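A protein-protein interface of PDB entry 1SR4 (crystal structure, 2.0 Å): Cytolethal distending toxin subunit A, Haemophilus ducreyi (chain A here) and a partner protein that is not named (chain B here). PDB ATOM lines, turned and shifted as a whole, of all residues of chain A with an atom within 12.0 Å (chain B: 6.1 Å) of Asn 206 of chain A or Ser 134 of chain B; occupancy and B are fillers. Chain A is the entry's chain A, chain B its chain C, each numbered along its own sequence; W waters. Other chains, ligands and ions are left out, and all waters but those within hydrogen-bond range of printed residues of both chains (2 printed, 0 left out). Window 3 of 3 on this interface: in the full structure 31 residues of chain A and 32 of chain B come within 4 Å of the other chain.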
ATOM      1  N   LEU A  40      17.899  25.243  19.422  1.00  0.00           N
ATOM      2  CA  LEU A  40      18.955  24.674  20.301  1.00  0.00           C
ATOM      3  C   LEU A  40      18.852  23.143  20.288  1.00  0.00           C
ATOM      4  O   LEU A  40      17.863  22.582  19.815  1.00  0.00           O
ATOM      5  CB  LEU A  40      18.780  25.194  21.725  1.00  0.00           C
ATOM      6  CG  LEU A  40      19.980  24.992  22.642  1.00  0.00           C
ATOM      7  CD1 LEU A  40      21.051  26.014  22.269  1.00  0.00           C
ATOM      8  CD2 LEU A  40      19.571  25.151  24.091  1.00  0.00           C
ATOM      9  N   LEU A  42      18.206  19.519  21.814  1.00  0.00           N
ATOM     10  CA  LEU A  42      17.530  18.879  22.943  1.00  0.00           C
ATOM     11  C   LEU A  42      18.434  17.775  23.509  1.00  0.00           C
ATOM     12  O   LEU A  42      18.279  17.361  24.659  1.00  0.00           O
ATOM     13  CB  LEU A  42      16.160  18.318  22.523  1.00  0.00           C
ATOM     14  CG  LEU A  42      14.996  19.329  22.578  1.00  0.00           C
ATOM     15  CD1 LEU A  42      15.345  20.548  21.734  1.00  0.00           C
ATOM     16  CD2 LEU A  42      13.709  18.697  22.066  1.00  0.00           C
ATOM     17  N   GLN A  51      16.081  22.874  27.858  1.00  0.00           N
ATOM     18  CA  GLN A  51      15.596  23.976  27.048  1.00  0.00           C
ATOM     19  C   GLN A  51      14.981  25.010  27.978  1.00  0.00           C
ATOM     20  O   GLN A  51      14.629  24.712  29.118  1.00  0.00           O
ATOM     21  CB  GLN A  51      14.550  23.498  26.035  1.00  0.00           C
ATOM     22  CG  GLN A  51      15.102  22.468  25.061  1.00  0.00           C
ATOM     23  CD  GLN A  51      16.256  23.023  24.243  1.00  0.00           C
ATOM     24  OE1 GLN A  51      16.051  23.821  23.330  1.00  0.00           O
ATOM     25  NE2 GLN A  51      17.478  22.618  24.581  1.00  0.00           N
ATOM     26  N   VAL A  52      14.883  26.232  27.485  1.00  0.00           N
ATOM     27  CA  VAL A  52      14.302  27.322  28.247  1.00  0.00           C
ATOM     28  C   VAL A  52      12.769  27.218  28.295  1.00  0.00           C
ATOM     29  O   VAL A  52      12.130  27.087  27.259  1.00  0.00           O
ATOM     30  CB  VAL A  52      14.666  28.686  27.600  1.00  0.00           C
ATOM     31  CG1 VAL A  52      13.987  29.836  28.360  1.00  0.00           C
ATOM     32  CG2 VAL A  52      16.175  28.871  27.594  1.00  0.00           C
ATOM     33  N   LEU A  53      12.196  27.250  29.499  1.00  0.00           N
ATOM     34  CA  LEU A  53      10.732  27.254  29.707  1.00  0.00           C
ATOM     35  C   LEU A  53      10.577  27.814  31.120  1.00  0.00           C
ATOM     36  O   LEU A  53      10.481  27.069  32.087  1.00  0.00           O
ATOM     37  CB  LEU A  53      10.108  25.853  29.610  1.00  0.00           C
ATOM     38  CG  LEU A  53       8.641  25.890  29.128  1.00  0.00           C
ATOM     39  CD1 LEU A  53       8.040  24.500  29.087  1.00  0.00           C
ATOM     40  CD2 LEU A  53       7.811  26.767  30.072  1.00  0.00           C
ATOM     41  N   PRO A  54      10.540  29.150  31.242  1.00  0.00           N
ATOM     42  CA  PRO A  54      10.422  29.905  32.495  1.00  0.00           C
ATOM     43  C   PRO A  54       9.296  29.490  33.438  1.00  0.00           C
ATOM     44  O   PRO A  54       8.152  29.337  33.018  1.00  0.00           O
ATOM     45  CB  PRO A  54      10.236  31.355  32.023  1.00  0.00           C
ATOM     46  CG  PRO A  54      10.679  31.351  30.580  1.00  0.00           C
ATOM     47  CD  PRO A  54      10.218  30.015  30.093  1.00  0.00           C
ATOM     48  N   SER A  58       4.772  32.053  36.310  1.00  0.00           N
ATOM     49  CA  SER A  58       3.702  31.378  37.028  1.00  0.00           C
ATOM     50  C   SER A  58       3.418  32.043  38.362  1.00  0.00           C
ATOM     51  O   SER A  58       2.329  31.888  38.927  1.00  0.00           O
ATOM     52  CB  SER A  58       4.082  29.915  37.313  1.00  0.00           C
ATOM     53  OG  SER A  58       4.280  29.193  36.110  1.00  0.00           O
ATOM     54  N   ALA A 202       3.621  34.361  27.238  1.00  0.00           N
ATOM     55  CA  ALA A 202       3.271  33.054  27.795  1.00  0.00           C
ATOM     56  C   ALA A 202       3.904  31.939  26.986  1.00  0.00           C
ATOM     57  O   ALA A 202       4.005  32.038  25.768  1.00  0.00           O
ATOM     58  CB  ALA A 202       1.746  32.890  27.788  1.00  0.00           C
ATOM     59  N   THR A 203       4.336  30.882  27.662  1.00  0.00           N
ATOM     60  CA  THR A 203       4.948  29.757  26.978  1.00  0.00           C
ATOM     61  C   THR A 203       3.982  28.581  27.107  1.00  0.00           C
ATOM     62  O   THR A 203       3.564  28.244  28.215  1.00  0.00           O
ATOM     63  CB  THR A 203       6.327  29.393  27.619  1.00  0.00           C
ATOM     64  OG1 THR A 203       7.202  30.531  27.559  1.00  0.00           O
ATOM     65  CG2 THR A 203       6.980  28.221  26.881  1.00  0.00           C
ATOM     66  N   ALA A 204       3.603  27.978  25.978  1.00  0.00           N
ATOM     67  CA  ALA A 204       2.695  26.823  25.989  1.00  0.00           C
ATOM     68  C   ALA A 204       3.368  25.629  26.662  1.00  0.00           C
ATOM     69  O   ALA A 204       4.547  25.345  26.415  1.00  0.00           O
ATOM     70  CB  ALA A 204       2.285  26.450  24.558  1.00  0.00           C
ATOM     71  N   VAL A 205       2.616  24.923  27.498  1.00  0.00           N
ATOM     72  CA  VAL A 205       3.153  23.788  28.226  1.00  0.00           C
ATOM     73  C   VAL A 205       2.451  22.480  27.896  1.00  0.00           C
ATOM     74  O   VAL A 205       2.586  21.505  28.627  1.00  0.00           O
ATOM     75  CB  VAL A 205       3.083  24.017  29.755  1.00  0.00           C
ATOM     76  CG1 VAL A 205       3.973  25.164  30.144  1.00  0.00           C
ATOM     77  CG2 VAL A 205       1.642  24.291  30.186  1.00  0.00           C
ATOM     78  N   ASN A 206       1.717  22.467  26.785  1.00  0.00           N
ATOM     79  CA  ASN A 206       1.002  21.276  26.329  1.00  0.00           C
ATOM     80  C   ASN A 206       1.985  20.179  25.924  1.00  0.00           C
ATOM     81  O   ASN A 206       3.121  20.519  25.548  1.00  0.00           O
ATOM     82  CB  ASN A 206       0.101  21.621  25.128  1.00  0.00           C
ATOM     83  CG  ASN A 206       0.858  22.321  23.980  1.00  0.00           C
ATOM     84  OD1 ASN A 206       1.595  23.286  24.193  1.00  0.00           O
ATOM     85  ND2 ASN A 206       0.645  21.842  22.756  1.00  0.00           N
ATOM     86  OXT ASN A 206       1.602  18.994  25.968  1.00  0.00           O
ATOM     87  N   ARG B  60      -4.685  17.694  17.830  1.00  0.00           N
ATOM     88  CA  ARG B  60      -5.025  18.131  19.186  1.00  0.00           C
ATOM     89  C   ARG B  60      -3.829  18.728  19.920  1.00  0.00           C
ATOM     90  O   ARG B  60      -3.989  19.554  20.811  1.00  0.00           O
ATOM     91  CB  ARG B  60      -5.652  16.989  19.994  1.00  0.00           C
ATOM     92  CG  ARG B  60      -6.130  17.405  21.397  1.00  0.00           C
ATOM     93  CD  ARG B  60      -7.096  16.376  21.965  1.00  0.00           C
ATOM     94  NE  ARG B  60      -6.467  15.075  22.190  1.00  0.00           N
ATOM     95  CZ  ARG B  60      -5.613  14.831  23.176  1.00  0.00           C
ATOM     96  NH1 ARG B  60      -5.286  15.809  24.019  1.00  0.00           N
ATOM     97  NH2 ARG B  60      -5.106  13.610  23.341  1.00  0.00           N
ATOM     98  N   ASP B  61      -2.631  18.290  19.569  1.00  0.00           N
ATOM     99  CA  ASP B  61      -1.436  18.887  20.152  1.00  0.00           C
ATOM    100  C   ASP B  61      -1.495  18.889  21.683  1.00  0.00           C
ATOM    101  O   ASP B  61      -1.052  19.841  22.335  1.00  0.00           O
ATOM    102  CB  ASP B  61      -1.327  20.318  19.592  1.00  0.00           C
ATOM    103  CG  ASP B  61       0.053  20.948  19.776  1.00  0.00           C
ATOM    104  OD1 ASP B  61       1.033  20.216  19.999  1.00  0.00           O
ATOM    105  OD2 ASP B  61       0.157  22.194  19.668  1.00  0.00           O
ATOM    106  N   GLY B  62      -2.049  17.823  22.253  1.00  0.00           N
ATOM    107  CA  GLY B  62      -2.134  17.719  23.700  1.00  0.00           C
ATOM    108  C   GLY B  62      -3.036  18.705  24.437  1.00  0.00           C
ATOM    109  O   GLY B  62      -2.976  18.788  25.660  1.00  0.00           O
ATOM    110  N   GLY B  63      -3.871  19.449  23.718  1.00  0.00           N
ATOM    111  CA  GLY B  63      -4.769  20.380  24.387  1.00  0.00           C
ATOM    112  C   GLY B  63      -6.087  19.707  24.749  1.00  0.00           C
ATOM    113  O   GLY B  63      -6.211  18.480  24.634  1.00  0.00           O
ATOM    114  N   ILE B  98      -5.063  25.223  25.035  1.00  0.00           N
ATOM    115  CA  ILE B  98      -3.635  24.940  25.210  1.00  0.00           C
ATOM    116  C   ILE B  98      -3.184  25.700  26.473  1.00  0.00           C
ATOM    117  O   ILE B  98      -3.182  26.926  26.484  1.00  0.00           O
ATOM    118  CB  ILE B  98      -2.803  25.494  24.003  1.00  0.00           C
ATOM    119  CG1 ILE B  98      -3.239  24.830  22.686  1.00  0.00           C
ATOM    120  CG2 ILE B  98      -1.300  25.332  24.270  1.00  0.00           C
ATOM    121  CD1 ILE B  98      -3.196  23.288  22.677  1.00  0.00           C
ATOM    122  N   PRO B  99      -2.803  24.985  27.539  1.00  0.00           N
ATOM    123  CA  PRO B  99      -2.360  25.660  28.765  1.00  0.00           C
ATOM    124  C   PRO B  99      -0.975  26.288  28.587  1.00  0.00           C
ATOM    125  O   PRO B  99      -0.212  25.893  27.702  1.00  0.00           O
ATOM    126  CB  PRO B  99      -2.358  24.534  29.811  1.00  0.00           C
ATOM    127  CG  PRO B  99      -1.965  23.327  29.005  1.00  0.00           C
ATOM    128  CD  PRO B  99      -2.737  23.514  27.676  1.00  0.00           C
ATOM    129  N   THR B 100      -0.661  27.261  29.440  1.00  0.00           N
ATOM    130  CA  THR B 100       0.626  27.963  29.395  1.00  0.00           C
ATOM    131  C   THR B 100       1.199  28.104  30.804  1.00  0.00           C
ATOM    132  O   THR B 100       0.524  27.777  31.792  1.00  0.00           O
ATOM    133  CB  THR B 100       0.478  29.392  28.841  1.00  0.00           C
ATOM    134  OG1 THR B 100      -0.217  30.199  29.795  1.00  0.00           O
ATOM    135  CG2 THR B 100      -0.279  29.392  27.533  1.00  0.00           C
ATOM    136  N   LYS B 108      -6.918  26.957  19.820  1.00  0.00           N
ATOM    137  CA  LYS B 108      -6.864  26.582  18.414  1.00  0.00           C
ATOM    138  C   LYS B 108      -8.195  25.983  17.999  1.00  0.00           C
ATOM    139  O   LYS B 108      -8.995  25.583  18.856  1.00  0.00           O
ATOM    140  CB  LYS B 108      -5.747  25.550  18.171  1.00  0.00           C
ATOM    141  CG  LYS B 108      -4.372  26.044  18.584  1.00  0.00           C
ATOM    142  CD  LYS B 108      -3.265  25.397  17.773  1.00  0.00           C
ATOM    143  CE  LYS B 108      -2.753  24.131  18.412  1.00  0.00           C
ATOM    144  NZ  LYS B 108      -1.598  23.582  17.627  1.00  0.00           N
ATOM    145  N   GLY B 131       3.475  24.533  13.502  1.00  0.00           N
ATOM    146  CA  GLY B 131       3.164  23.189  13.953  1.00  0.00           C
ATOM    147  C   GLY B 131       2.867  23.235  15.445  1.00  0.00           C
ATOM    148  O   GLY B 131       2.328  24.221  15.944  1.00  0.00           O
ATOM    149  N   SER B 132       3.211  22.179  16.166  1.00  0.00           N
ATOM    150  CA  SER B 132       2.956  22.139  17.601  1.00  0.00           C
ATOM    151  C   SER B 132       3.408  23.425  18.298  1.00  0.00           C
ATOM    152  O   SER B 132       4.487  23.966  18.007  1.00  0.00           O
ATOM    153  CB  SER B 132       3.680  20.946  18.231  1.00  0.00           C
ATOM    154  OG  SER B 132       3.463  20.909  19.628  1.00  0.00           O
ATOM    155  N   VAL B 133       2.582  23.923  19.214  1.00  0.00           N
ATOM    156  CA  VAL B 133       2.947  25.126  19.942  1.00  0.00           C
ATOM    157  C   VAL B 133       3.716  24.802  21.229  1.00  0.00           C
ATOM    158  O   VAL B 133       4.110  25.708  21.955  1.00  0.00           O
ATOM    159  CB  VAL B 133       1.696  25.973  20.312  1.00  0.00           C
ATOM    160  CG1 VAL B 133       1.011  26.474  19.051  1.00  0.00           C
ATOM    161  CG2 VAL B 133       0.720  25.137  21.155  1.00  0.00           C
ATOM    162  N   SER B 134       3.959  23.524  21.504  1.00  0.00           N
ATOM    163  CA  SER B 134       4.642  23.152  22.751  1.00  0.00           C
ATOM    164  C   SER B 134       5.957  23.863  22.990  1.00  0.00           C
ATOM    165  O   SER B 134       6.834  23.843  22.138  1.00  0.00           O
ATOM    166  CB  SER B 134       4.932  21.649  22.804  1.00  0.00           C
ATOM    167  OG  SER B 134       3.746  20.899  22.803  1.00  0.00           O
ATOM    168  N   GLY B 135       6.089  24.477  24.164  1.00  0.00           N
ATOM    169  CA  GLY B 135       7.328  25.146  24.512  1.00  0.00           C
ATOM    170  C   GLY B 135       7.640  26.438  23.789  1.00  0.00           C
ATOM    171  O   GLY B 135       8.712  26.995  23.983  1.00  0.00           O
ATOM    172  N   ARG B 136       6.726  26.916  22.950  1.00  0.00           N
ATOM    173  CA  ARG B 136       6.958  28.164  22.236  1.00  0.00           C
ATOM    174  C   ARG B 136       6.331  29.299  23.041  1.00  0.00           C
ATOM    175  O   ARG B 136       5.399  29.080  23.831  1.00  0.00           O
ATOM    176  CB  ARG B 136       6.361  28.098  20.830  1.00  0.00           C
ATOM    177  CG  ARG B 136       7.138  27.176  19.874  1.00  0.00           C
ATOM    178  CD  ARG B 136       6.334  26.844  18.617  1.00  0.00           C
ATOM    179  NE  ARG B 136       5.811  28.028  17.930  1.00  0.00           N
ATOM    180  CZ  ARG B 136       4.801  27.991  17.066  1.00  0.00           C
ATOM    181  NH1 ARG B 136       4.205  26.837  16.789  1.00  0.00           N
ATOM    182  NH2 ARG B 136       4.380  29.100  16.475  1.00  0.00           N
ATOM    183  N   PHE B 138       4.504  33.192  23.278  1.00  0.00           N
ATOM    184  CA  PHE B 138       3.527  33.977  22.540  1.00  0.00           C
ATOM    185  C   PHE B 138       3.158  35.313  23.190  1.00  0.00           C
ATOM    186  O   PHE B 138       3.087  35.418  24.414  1.00  0.00           O
ATOM    187  CB  PHE B 138       2.253  33.125  22.394  1.00  0.00           C
ATOM    188  CG  PHE B 138       2.458  31.853  21.601  1.00  0.00           C
ATOM    189  CD1 PHE B 138       2.309  31.850  20.214  1.00  0.00           C
ATOM    190  CD2 PHE B 138       2.802  30.668  22.239  1.00  0.00           C
ATOM    191  CE1 PHE B 138       2.497  30.676  19.473  1.00  0.00           C
ATOM    192  CE2 PHE B 138       2.994  29.485  21.505  1.00  0.00           C
ATOM    193  CZ  PHE B 138       2.840  29.490  20.125  1.00  0.00           C
HETATM  194  O   HOH W   1      10.387  25.702  25.725  1.00  0.00           O
HETATM  195  O   HOH W   2       4.797  18.389  24.877  1.00  0.00           O
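Of the 15 printed residues of chain B, 9 touch a printed residue of chain A.
Printed residues of chain B that touch a printed residue of chain A: Asp 61, Ile 98, Pro 99, Thr 100, Val 133, Ser 134, Gly 135, Arg 136 and Phe 138.
Hydrophobic or aromatic side chains of chain B within 4 Å of the printed part of chain A: Ile 98, Pro 99, Val 133 and Phe 138.
Among the printed residues, 18 pairs touch across the chains.
The side-chain carboxylate (OD2) of Asp 61 of chain B sits at hydrogen-bond distance from the backbone NH (N) of Val 133 of chain B, at 3.0 Å.
The guanidinium group of Arg 136 of chain B is in hydrogen-bond range of the backbone carbonyl oxygen of Gly 131 of chain B (3.3 Å).
OD2 of Asp 61 of chain B is in salt-bridge range of NZ of Lys 108 of chain B (3.0 Å).
The backbone carbonyl oxygen of Ser 132 of chain B lies within hydrogen-bond range of the guanidinium group of Arg 136 of chain B (3.1 Å).
OD1 of Asp 61 of chain B is in hydrogen-bond range of OG of Ser 132 of chain B (2.6 Å).
OG of Ser 134 of chain B is in hydrogen-bond range of OG of Ser 132 of chain B (3.2 Å).
Asn 206 of chain A touches four residues of chain B.
Of the printed residues of chain A, Ser 134 of chain B touches Ala 204 and Asn 206.
Pro 99 of chain B touches two residues of chain A.
Gly 135 of chain B touches just these residues of chain A: Thr 203 and Ala 204.
Of the printed residues of chain A, Thr 100 of chain B touches Ala 202, Thr 203 and Val 205.
Of the printed residues of chain B, Thr 203 of chain A touches Thr 100, Gly 135 and Arg 136.
Printed residues of chain A within 4 Å of Phe 138 of chain B: Ala 202.
Printed residues of chain B within 4 Å of Val 205 of chain A: Pro 99 (3.0 Å) and Thr 100 (3.8 Å).
Val 52 of chain A touches none of the printed residues of chain B.
The nearest residue of chain B that does not touch Asn 206 of chain A is Pro 99 of chain B (4.04 Å).
The nearest printed residue of chain B that does not touch Thr 203 of chain A is Pro 99 of chain B (4.5 Å).
Among the printed residues, pairs that only touch across the chains: Ala 202 of chain A with Thr 100 of chain B (3.9 Å), Ala 202 of chain A with Arg 136 of chain B (3.8 Å), Thr 203 of chain A with Thr 100 of chain B (3.2 Å), Thr 203 of chain A with Gly 135 of chain B (3.6 Å), Thr 203 of chain A with Arg 136 of chain B (3.3 Å), Ala 204 of chain A with Ile 98 of chain B (3.8 Å), Ala 204 of chain A with Pro 99 of chain B (3.5 Å), Ala 204 of chain A with Val 133 of chain B (3.3 Å), Ala 204 of chain A with Ser 134 of chain B (3.99 Å), Val 205 of chain A with Thr 100 of chain B (3.8 Å), Asn 206 of chain A with Ile 98 of chain B (3.5 Å) and Asn 206 of chain A with Val 133 of chain B (3.7 Å).
O of Ala 204 of chain A sits at hydrogen-bond distance from N of Gly 135 of chain B (2.9 Å).
The backbone carbonyl oxygen (O) of Pro 99 of chain B is in hydrogen-bond range of the backbone NH (N) of Val 205 of chain A, 3.0 Å away.
ND2 of Asn 206 of chain A is in hydrogen-bond range of O of Asp 61 of chain B.
The backbone NH of Phe 138 of chain B sits at hydrogen-bond distance from the backbone carbonyl oxygen of Ala 202 of chain A (2.8 Å).
The backbone NH (N) of Ala 204 of chain A sits at hydrogen-bond distance from the backbone carbonyl oxygen (O) of Arg 136 of chain B (3.0 Å).
OG of Ser 134 of chain B lies within hydrogen-bond range of O of Asn 206 of chain A, 2.8 Å away.
Water W1 lies within hydrogen-bond range of O of Val 52 of chain A (2.7 Å) and O of Gly 135 of chain B (2.7 Å).
Water W2 bridges the chain-end carboxylate of Asn 206 of chain A and the side-chain hydroxyl of Ser 134 of chain B.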
